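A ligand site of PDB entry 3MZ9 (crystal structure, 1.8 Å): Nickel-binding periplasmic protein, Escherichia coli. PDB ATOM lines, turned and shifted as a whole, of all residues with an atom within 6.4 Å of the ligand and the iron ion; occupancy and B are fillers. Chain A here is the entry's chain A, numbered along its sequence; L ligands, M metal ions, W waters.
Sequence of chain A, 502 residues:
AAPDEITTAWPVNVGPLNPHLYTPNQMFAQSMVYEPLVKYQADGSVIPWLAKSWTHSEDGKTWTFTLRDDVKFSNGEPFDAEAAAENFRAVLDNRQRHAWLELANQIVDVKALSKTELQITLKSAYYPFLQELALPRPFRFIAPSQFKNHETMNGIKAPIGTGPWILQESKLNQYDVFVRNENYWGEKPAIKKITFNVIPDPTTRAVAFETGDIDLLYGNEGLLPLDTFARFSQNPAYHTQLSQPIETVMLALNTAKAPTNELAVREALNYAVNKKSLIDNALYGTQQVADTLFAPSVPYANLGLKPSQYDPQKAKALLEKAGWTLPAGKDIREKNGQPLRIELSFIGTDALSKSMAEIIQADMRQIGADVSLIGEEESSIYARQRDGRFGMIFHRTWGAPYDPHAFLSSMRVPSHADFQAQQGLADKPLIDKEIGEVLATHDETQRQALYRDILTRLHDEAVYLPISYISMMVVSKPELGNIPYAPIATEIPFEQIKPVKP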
ATOM      1  N   TYR A  22      -6.487 -28.336 -11.985  1.00  0.00           N
ATOM      2  CA  TYR A  22      -7.463 -27.262 -11.735  1.00  0.00           C
ATOM      3  C   TYR A  22      -8.095 -27.465 -10.369  1.00  0.00           C
ATOM      4  O   TYR A  22      -7.356 -27.658  -9.401  1.00  0.00           O
ATOM      5  CB  TYR A  22      -8.475 -27.193 -12.910  1.00  0.00           C
ATOM      6  CG  TYR A  22      -7.765 -26.971 -14.242  1.00  0.00           C
ATOM      7  CD1 TYR A  22      -7.475 -28.059 -15.088  1.00  0.00           C
ATOM      8  CD2 TYR A  22      -7.301 -25.714 -14.604  1.00  0.00           C
ATOM      9  CE1 TYR A  22      -6.788 -27.872 -16.288  1.00  0.00           C
ATOM     10  CE2 TYR A  22      -6.622 -25.501 -15.824  1.00  0.00           C
ATOM     11  CZ  TYR A  22      -6.372 -26.594 -16.651  1.00  0.00           C
ATOM     12  OH  TYR A  22      -5.711 -26.378 -17.834  1.00  0.00           O
ATOM     13  N   THR A  23      -9.420 -27.403 -10.236  1.00  0.00           N
ATOM     14  CA  THR A  23     -10.076 -27.691  -8.945  1.00  0.00           C
ATOM     15  C   THR A  23      -9.520 -28.955  -8.254  1.00  0.00           C
ATOM     16  O   THR A  23      -9.276 -29.986  -8.928  1.00  0.00           O
ATOM     17  CB  THR A  23     -11.664 -27.746  -9.058  1.00  0.00           C
ATOM     18  OG1 THR A  23     -12.209 -28.199  -7.806  1.00  0.00           O
ATOM     19  CG2 THR A  23     -12.102 -28.708 -10.128  1.00  0.00           C
ATOM     20  N   MET A  27      -5.833 -20.825  -7.992  1.00  0.00           N
ATOM     21  CA  MET A  27      -4.876 -20.229  -8.936  1.00  0.00           C
ATOM     22  C   MET A  27      -3.915 -19.242  -8.295  1.00  0.00           C
ATOM     23  O   MET A  27      -2.730 -19.240  -8.648  1.00  0.00           O
ATOM     24  CB  MET A  27      -5.587 -19.545 -10.095  1.00  0.00           C
ATOM     25  CG  MET A  27      -6.529 -20.465 -10.860  1.00  0.00           C
ATOM     26  SD  MET A  27      -7.585 -19.531 -11.958  1.00  0.00           S
ATOM     27  CE  MET A  27      -6.331 -19.072 -13.164  1.00  0.00           C
ATOM     28  N   ARG A  97      -7.538 -32.591 -20.731  1.00  0.00           N
ATOM     29  CA  ARG A  97      -7.981 -31.741 -19.636  1.00  0.00           C
ATOM     30  C   ARG A  97      -7.654 -30.260 -19.911  1.00  0.00           C
ATOM     31  O   ARG A  97      -8.214 -29.377 -19.255  1.00  0.00           O
ATOM     32  CB  ARG A  97      -7.365 -32.232 -18.328  1.00  0.00           C
ATOM     33  CG  ARG A  97      -7.762 -31.446 -17.077  1.00  0.00           C
ATOM     34  CD  ARG A  97      -8.820 -32.128 -16.180  1.00  0.00           C
ATOM     35  NE  ARG A  97      -8.558 -31.774 -14.768  1.00  0.00           N
ATOM     36  CZ  ARG A  97      -9.299 -32.075 -13.706  1.00  0.00           C
ATOM     37  NH1 ARG A  97     -10.430 -32.770 -13.808  1.00  0.00           N
ATOM     38  NH2 ARG A  97      -8.897 -31.652 -12.507  1.00  0.00           N
ATOM     39  N   TRP A 100      -9.531 -26.453 -23.340  1.00  0.00           N
ATOM     40  CA  TRP A 100      -9.952 -25.071 -23.298  1.00  0.00           C
ATOM     41  C   TRP A 100      -8.828 -24.137 -23.767  1.00  0.00           C
ATOM     42  O   TRP A 100      -9.102 -23.071 -24.265  1.00  0.00           O
ATOM     43  CB  TRP A 100     -10.421 -24.672 -21.889  1.00  0.00           C
ATOM     44  CG  TRP A 100      -9.286 -24.611 -20.896  1.00  0.00           C
ATOM     45  CD1 TRP A 100      -8.823 -25.641 -20.109  1.00  0.00           C
ATOM     46  CD2 TRP A 100      -8.477 -23.480 -20.599  1.00  0.00           C
ATOM     47  NE1 TRP A 100      -7.764 -25.201 -19.340  1.00  0.00           N
ATOM     48  CE2 TRP A 100      -7.521 -23.883 -19.626  1.00  0.00           C
ATOM     49  CE3 TRP A 100      -8.445 -22.161 -21.065  1.00  0.00           C
ATOM     50  CZ2 TRP A 100      -6.566 -23.001 -19.093  1.00  0.00           C
ATOM     51  CZ3 TRP A 100      -7.493 -21.299 -20.542  1.00  0.00           C
ATOM     52  CH2 TRP A 100      -6.559 -21.725 -19.570  1.00  0.00           C
ATOM     53  N   PRO A 136      -1.192 -18.510 -15.089  1.00  0.00           N
ATOM     54  CA  PRO A 136      -0.991 -19.201 -13.802  1.00  0.00           C
ATOM     55  C   PRO A 136      -0.847 -20.727 -13.945  1.00  0.00           C
ATOM     56  O   PRO A 136      -0.048 -21.340 -13.198  1.00  0.00           O
ATOM     57  CB  PRO A 136      -2.277 -18.886 -13.022  1.00  0.00           C
ATOM     58  CG  PRO A 136      -2.696 -17.547 -13.566  1.00  0.00           C
ATOM     59  CD  PRO A 136      -2.331 -17.556 -15.012  1.00  0.00           C
ATOM     60  N   ARG A 137      -1.584 -21.317 -14.895  1.00  0.00           N
ATOM     61  CA  ARG A 137      -1.560 -22.761 -15.168  1.00  0.00           C
ATOM     62  C   ARG A 137      -2.031 -23.006 -16.609  1.00  0.00           C
ATOM     63  O   ARG A 137      -2.789 -22.182 -17.179  1.00  0.00           O
ATOM     64  CB  ARG A 137      -2.407 -23.534 -14.131  1.00  0.00           C
ATOM     65  CG  ARG A 137      -3.919 -23.186 -14.102  1.00  0.00           C
ATOM     66  CD  ARG A 137      -4.547 -23.508 -12.769  1.00  0.00           C
ATOM     67  NE  ARG A 137      -5.997 -23.278 -12.829  1.00  0.00           N
ATOM     68  CZ  ARG A 137      -6.838 -23.464 -11.813  1.00  0.00           C
ATOM     69  NH1 ARG A 137      -6.421 -23.854 -10.619  1.00  0.00           N
ATOM     70  NH2 ARG A 137      -8.134 -23.247 -12.026  1.00  0.00           N
ATOM     71  N   PRO A 138      -1.623 -24.134 -17.210  1.00  0.00           N
ATOM     72  CA  PRO A 138      -0.835 -25.203 -16.556  1.00  0.00           C
ATOM     73  C   PRO A 138       0.670 -25.175 -16.822  1.00  0.00           C
ATOM     74  O   PRO A 138       1.363 -26.065 -16.357  1.00  0.00           O
ATOM     75  CB  PRO A 138      -1.408 -26.454 -17.200  1.00  0.00           C
ATOM     76  CG  PRO A 138      -1.617 -25.989 -18.664  1.00  0.00           C
ATOM     77  CD  PRO A 138      -2.111 -24.555 -18.541  1.00  0.00           C
ATOM     78  N   GLU A 247     -12.974  -7.312 -15.657  1.00  0.00           N
ATOM     79  CA  GLU A 247     -13.708  -8.291 -16.491  1.00  0.00           C
ATOM     80  C   GLU A 247     -15.199  -8.011 -16.499  1.00  0.00           C
ATOM     81  O   GLU A 247     -15.687  -7.160 -15.748  1.00  0.00           O
ATOM     82  CB  GLU A 247     -13.448  -9.736 -16.051  1.00  0.00           C
ATOM     83  CG  GLU A 247     -14.011 -10.053 -14.674  1.00  0.00           C
ATOM     84  CD  GLU A 247     -13.189 -11.085 -13.914  1.00  0.00           C
ATOM     85  OE1 GLU A 247     -13.738 -11.625 -12.941  1.00  0.00           O
ATOM     86  OE2 GLU A 247     -12.031 -11.360 -14.272  1.00  0.00           O
ATOM     87  N   HIS A 395     -22.663 -15.375 -15.790  1.00  0.00           N
ATOM     88  CA  HIS A 395     -21.426 -15.795 -16.414  1.00  0.00           C
ATOM     89  C   HIS A 395     -20.481 -14.591 -16.339  1.00  0.00           C
ATOM     90  O   HIS A 395     -20.926 -13.446 -16.166  1.00  0.00           O
ATOM     91  CB  HIS A 395     -21.689 -16.240 -17.865  1.00  0.00           C
ATOM     92  CG  HIS A 395     -20.575 -17.027 -18.468  1.00  0.00           C
ATOM     93  ND1 HIS A 395     -19.846 -17.954 -17.752  1.00  0.00           N
ATOM     94  CD2 HIS A 395     -20.061 -17.046 -19.721  1.00  0.00           C
ATOM     95  CE1 HIS A 395     -18.927 -18.488 -18.537  1.00  0.00           C
ATOM     96  NE2 HIS A 395     -19.032 -17.949 -19.735  1.00  0.00           N
ATOM     97  N   THR A 397     -16.446 -13.041 -17.906  1.00  0.00           N
ATOM     98  CA  THR A 397     -15.214 -13.177 -18.668  1.00  0.00           C
ATOM     99  C   THR A 397     -14.021 -13.332 -17.728  1.00  0.00           C
ATOM    100  O   THR A 397     -14.182 -13.370 -16.520  1.00  0.00           O
ATOM    101  CB  THR A 397     -14.985 -12.047 -19.703  1.00  0.00           C
ATOM    102  OG1 THR A 397     -14.647 -10.812 -19.045  1.00  0.00           O
ATOM    103  CG2 THR A 397     -16.244 -11.868 -20.607  1.00  0.00           C
ATOM    104  N   TRP A 398     -12.832 -13.429 -18.292  1.00  0.00           N
ATOM    105  CA  TRP A 398     -11.723 -14.008 -17.540  1.00  0.00           C
ATOM    106  C   TRP A 398     -10.650 -13.020 -17.162  1.00  0.00           C
ATOM    107  O   TRP A 398      -9.775 -13.343 -16.365  1.00  0.00           O
ATOM    108  CB  TRP A 398     -11.129 -15.165 -18.359  1.00  0.00           C
ATOM    109  CG  TRP A 398     -12.043 -16.359 -18.482  1.00  0.00           C
ATOM    110  CD1 TRP A 398     -13.194 -16.601 -17.778  1.00  0.00           C
ATOM    111  CD2 TRP A 398     -11.844 -17.512 -19.329  1.00  0.00           C
ATOM    112  NE1 TRP A 398     -13.724 -17.831 -18.140  1.00  0.00           N
ATOM    113  CE2 TRP A 398     -12.917 -18.408 -19.082  1.00  0.00           C
ATOM    114  CE3 TRP A 398     -10.851 -17.881 -20.263  1.00  0.00           C
ATOM    115  CZ2 TRP A 398     -13.038 -19.637 -19.751  1.00  0.00           C
ATOM    116  CZ3 TRP A 398     -10.967 -19.112 -20.911  1.00  0.00           C
ATOM    117  CH2 TRP A 398     -12.053 -19.981 -20.654  1.00  0.00           C
ATOM    118  N   GLY A 399     -10.723 -11.813 -17.712  1.00  0.00           N
ATOM    119  CA  GLY A 399      -9.756 -10.781 -17.443  1.00  0.00           C
ATOM    120  C   GLY A 399      -8.477 -10.954 -18.252  1.00  0.00           C
ATOM    121  O   GLY A 399      -8.352 -11.901 -19.042  1.00  0.00           O
ATOM    122  N   TYR A 402      -6.420 -13.325 -20.589  1.00  0.00           N
ATOM    123  CA  TYR A 402      -7.371 -14.260 -21.205  1.00  0.00           C
ATOM    124  C   TYR A 402      -8.314 -13.582 -22.193  1.00  0.00           C
ATOM    125  O   TYR A 402      -8.693 -14.162 -23.203  1.00  0.00           O
ATOM    126  CB  TYR A 402      -8.247 -14.985 -20.176  1.00  0.00           C
ATOM    127  CG  TYR A 402      -7.515 -15.780 -19.118  1.00  0.00           C
ATOM    128  CD1 TYR A 402      -7.118 -15.168 -17.921  1.00  0.00           C
ATOM    129  CD2 TYR A 402      -7.239 -17.137 -19.284  1.00  0.00           C
ATOM    130  CE1 TYR A 402      -6.441 -15.892 -16.932  1.00  0.00           C
ATOM    131  CE2 TYR A 402      -6.568 -17.859 -18.316  1.00  0.00           C
ATOM    132  CZ  TYR A 402      -6.175 -17.242 -17.128  1.00  0.00           C
ATOM    133  OH  TYR A 402      -5.517 -17.995 -16.145  1.00  0.00           O
ATOM    134  N   SER A 410     -12.219 -20.677 -25.965  1.00  0.00           N
ATOM    135  CA  SER A 410     -13.005 -21.622 -25.186  1.00  0.00           C
ATOM    136  C   SER A 410     -14.483 -21.712 -25.618  1.00  0.00           C
ATOM    137  O   SER A 410     -15.177 -22.645 -25.226  1.00  0.00           O
ATOM    138  CB  SER A 410     -12.913 -21.334 -23.696  1.00  0.00           C
ATOM    139  OG  SER A 410     -13.777 -20.274 -23.336  1.00  0.00           O
ATOM    140  N   HIS A 416     -18.980 -26.416 -22.265  1.00  0.00           N
ATOM    141  CA  HIS A 416     -18.882 -25.180 -21.516  1.00  0.00           C
ATOM    142  C   HIS A 416     -20.016 -24.242 -21.870  1.00  0.00           C
ATOM    143  O   HIS A 416     -20.566 -24.310 -22.951  1.00  0.00           O
ATOM    144  CB  HIS A 416     -17.545 -24.500 -21.775  1.00  0.00           C
ATOM    145  CG  HIS A 416     -17.213 -23.456 -20.765  1.00  0.00           C
ATOM    146  ND1 HIS A 416     -17.235 -23.703 -19.408  1.00  0.00           N
ATOM    147  CD2 HIS A 416     -16.884 -22.153 -20.902  1.00  0.00           C
ATOM    148  CE1 HIS A 416     -16.921 -22.609 -18.754  1.00  0.00           C
ATOM    149  NE2 HIS A 416     -16.697 -21.642 -19.639  1.00  0.00           N
ATOM    150  N   THR A 490      -6.163 -12.998 -11.877  1.00  0.00           N
ATOM    151  CA  THR A 490      -6.293 -14.064 -10.870  1.00  0.00           C
ATOM    152  C   THR A 490      -5.154 -14.167  -9.872  1.00  0.00           C
ATOM    153  O   THR A 490      -5.188 -15.016  -8.983  1.00  0.00           O
ATOM    154  CB  THR A 490      -6.472 -15.454 -11.538  1.00  0.00           C
ATOM    155  OG1 THR A 490      -5.338 -15.742 -12.347  1.00  0.00           O
ATOM    156  CG2 THR A 490      -7.706 -15.449 -12.414  1.00  0.00           C
HETATM  157  C1  LIG L   1     -10.398 -18.809 -15.673  1.00  0.00           C
HETATM  158  C2  LIG L   1      -9.989 -17.496 -15.847  1.00  0.00           C
HETATM  159  C3  LIG L   1      -9.938 -16.629 -14.764  1.00  0.00           C
HETATM  160  C4  LIG L   1     -10.282 -17.096 -13.488  1.00  0.00           C
HETATM  161  C5  LIG L   1     -10.688 -18.413 -13.306  1.00  0.00           C
HETATM  162  C6  LIG L   1     -10.745 -19.268 -14.391  1.00  0.00           C
HETATM  163  O1  LIG L   1     -11.113 -20.570 -14.208  1.00  0.00           O
HETATM  164  C7  LIG L   1     -10.441 -19.663 -16.918  1.00  0.00           C
HETATM  165  N1  LIG L   1      -9.920 -20.995 -16.667  1.00  0.00           N
HETATM  166  C8  LIG L   1     -10.152 -21.694 -17.938  1.00  0.00           C
HETATM  167  C9  LIG L   1     -10.175 -23.200 -17.738  1.00  0.00           C
HETATM  168  N2  LIG L   1     -10.966 -23.555 -16.553  1.00  0.00           N
HETATM  169  C10 LIG L   1     -10.436 -24.875 -16.160  1.00  0.00           C
HETATM  170  C11 LIG L   1     -11.141 -25.390 -14.898  1.00  0.00           C
HETATM  171  C12 LIG L   1     -11.373 -26.761 -14.826  1.00  0.00           C
HETATM  172  C13 LIG L   1     -12.017 -27.312 -13.706  1.00  0.00           C
HETATM  173  C14 LIG L   1     -12.423 -26.481 -12.667  1.00  0.00           C
HETATM  174  C15 LIG L   1     -12.183 -25.106 -12.740  1.00  0.00           C
HETATM  175  C16 LIG L   1     -11.550 -24.577 -13.855  1.00  0.00           C
HETATM  176  O2  LIG L   1     -11.324 -23.235 -13.927  1.00  0.00           O
HETATM  177  C17 LIG L   1      -8.455 -20.828 -16.488  1.00  0.00           C
HETATM  178  C18 LIG L   1      -7.931 -21.780 -15.396  1.00  0.00           C
HETATM  179  O3  LIG L   1      -6.704 -21.781 -15.252  1.00  0.00           O
HETATM  180  C19 LIG L   1     -12.339 -23.810 -17.061  1.00  0.00           C
HETATM  181  O4  LIG L   1      -8.742 -22.440 -14.733  1.00  0.00           O
HETATM  182  C20 LIG L   1     -13.269 -22.605 -16.849  1.00  0.00           C
HETATM  183  O5  LIG L   1     -14.263 -22.581 -17.588  1.00  0.00           O
HETATM  184  O6  LIG L   1     -12.986 -21.748 -15.984  1.00  0.00           O
HETATM  185 FE    FE M   1     -10.911 -22.032 -15.056  1.00  0.00          FE
HETATM  186  O   HOH W   1     -15.685 -20.220 -17.579  1.00  0.00           O
HETATM  187  O   HOH W   2     -13.764 -23.630 -20.342  1.00  0.00           O
HETATM  188  O   HOH W   3      -4.954 -20.686 -16.534  1.00  0.00           O
HETATM  189  O   HOH W   4     -14.458 -19.767 -14.921  1.00  0.00           O
HETATM  190  O   HOH W   5     -10.266 -29.317 -16.929  1.00  0.00           O
HETATM  191  O   HOH W   6     -11.460 -21.455 -11.455  1.00  0.00           O
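The guanidinium group of Arg 137 lies within salt-bridge range of an oxygen (O3) of the ligand (2.9 Å). A ring nitrogen (NE2) of His 416 lies close to an oxygen (O5) of the ligand, 3.3 Å away.
No residue comes within 4 Å of the iron ion.
Water W3 lies within hydrogen-bond range of O3 of the ligand (2.4 Å), O of Arg 137 (2.7 Å) and OH of Tyr 402 (2.8 Å). Water W1 lies within hydrogen-bond range of NE2 of His 416, O5 of the ligand and NE1 of Trp 398.
Merely in contact with the ligand: Thr 490 (3.2 Å), Trp 100 (3.3 Å), Thr 23 (3.4 Å), Met 27 (3.4 Å), Tyr 22 (3.5 Å), Trp 398 (3.5 Å) and Tyr 402 (3.96 Å). Within 4 Å of the ligand: Tyr 22, Thr 23, Met 27, Trp 100, Arg 137, Trp 398, Tyr 402, His 416 and Thr 490.
NH2 of Arg 137 sits close to SD of Met 27, 3.8 Å away. The indole nitrogen (NE1) of Trp 100 lies within hydrogen-bond range of the side-chain hydroxyl (OH) of Tyr 22 (2.8 Å).
An oxygen (O2) of the ligand binds the iron ion (1.7 Å). The iron ion is bound by O1 of the ligand, 1.7 Å away. N2 of the ligand binds the iron ion (2.1 Å). A nitrogen (N1) of the ligand binds the iron ion (2.2 Å). O4 of the ligand binds the iron ion (2.2 Å). O6 of the ligand is bound to the iron ion. The iron ion has six donor atoms within binding distance.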
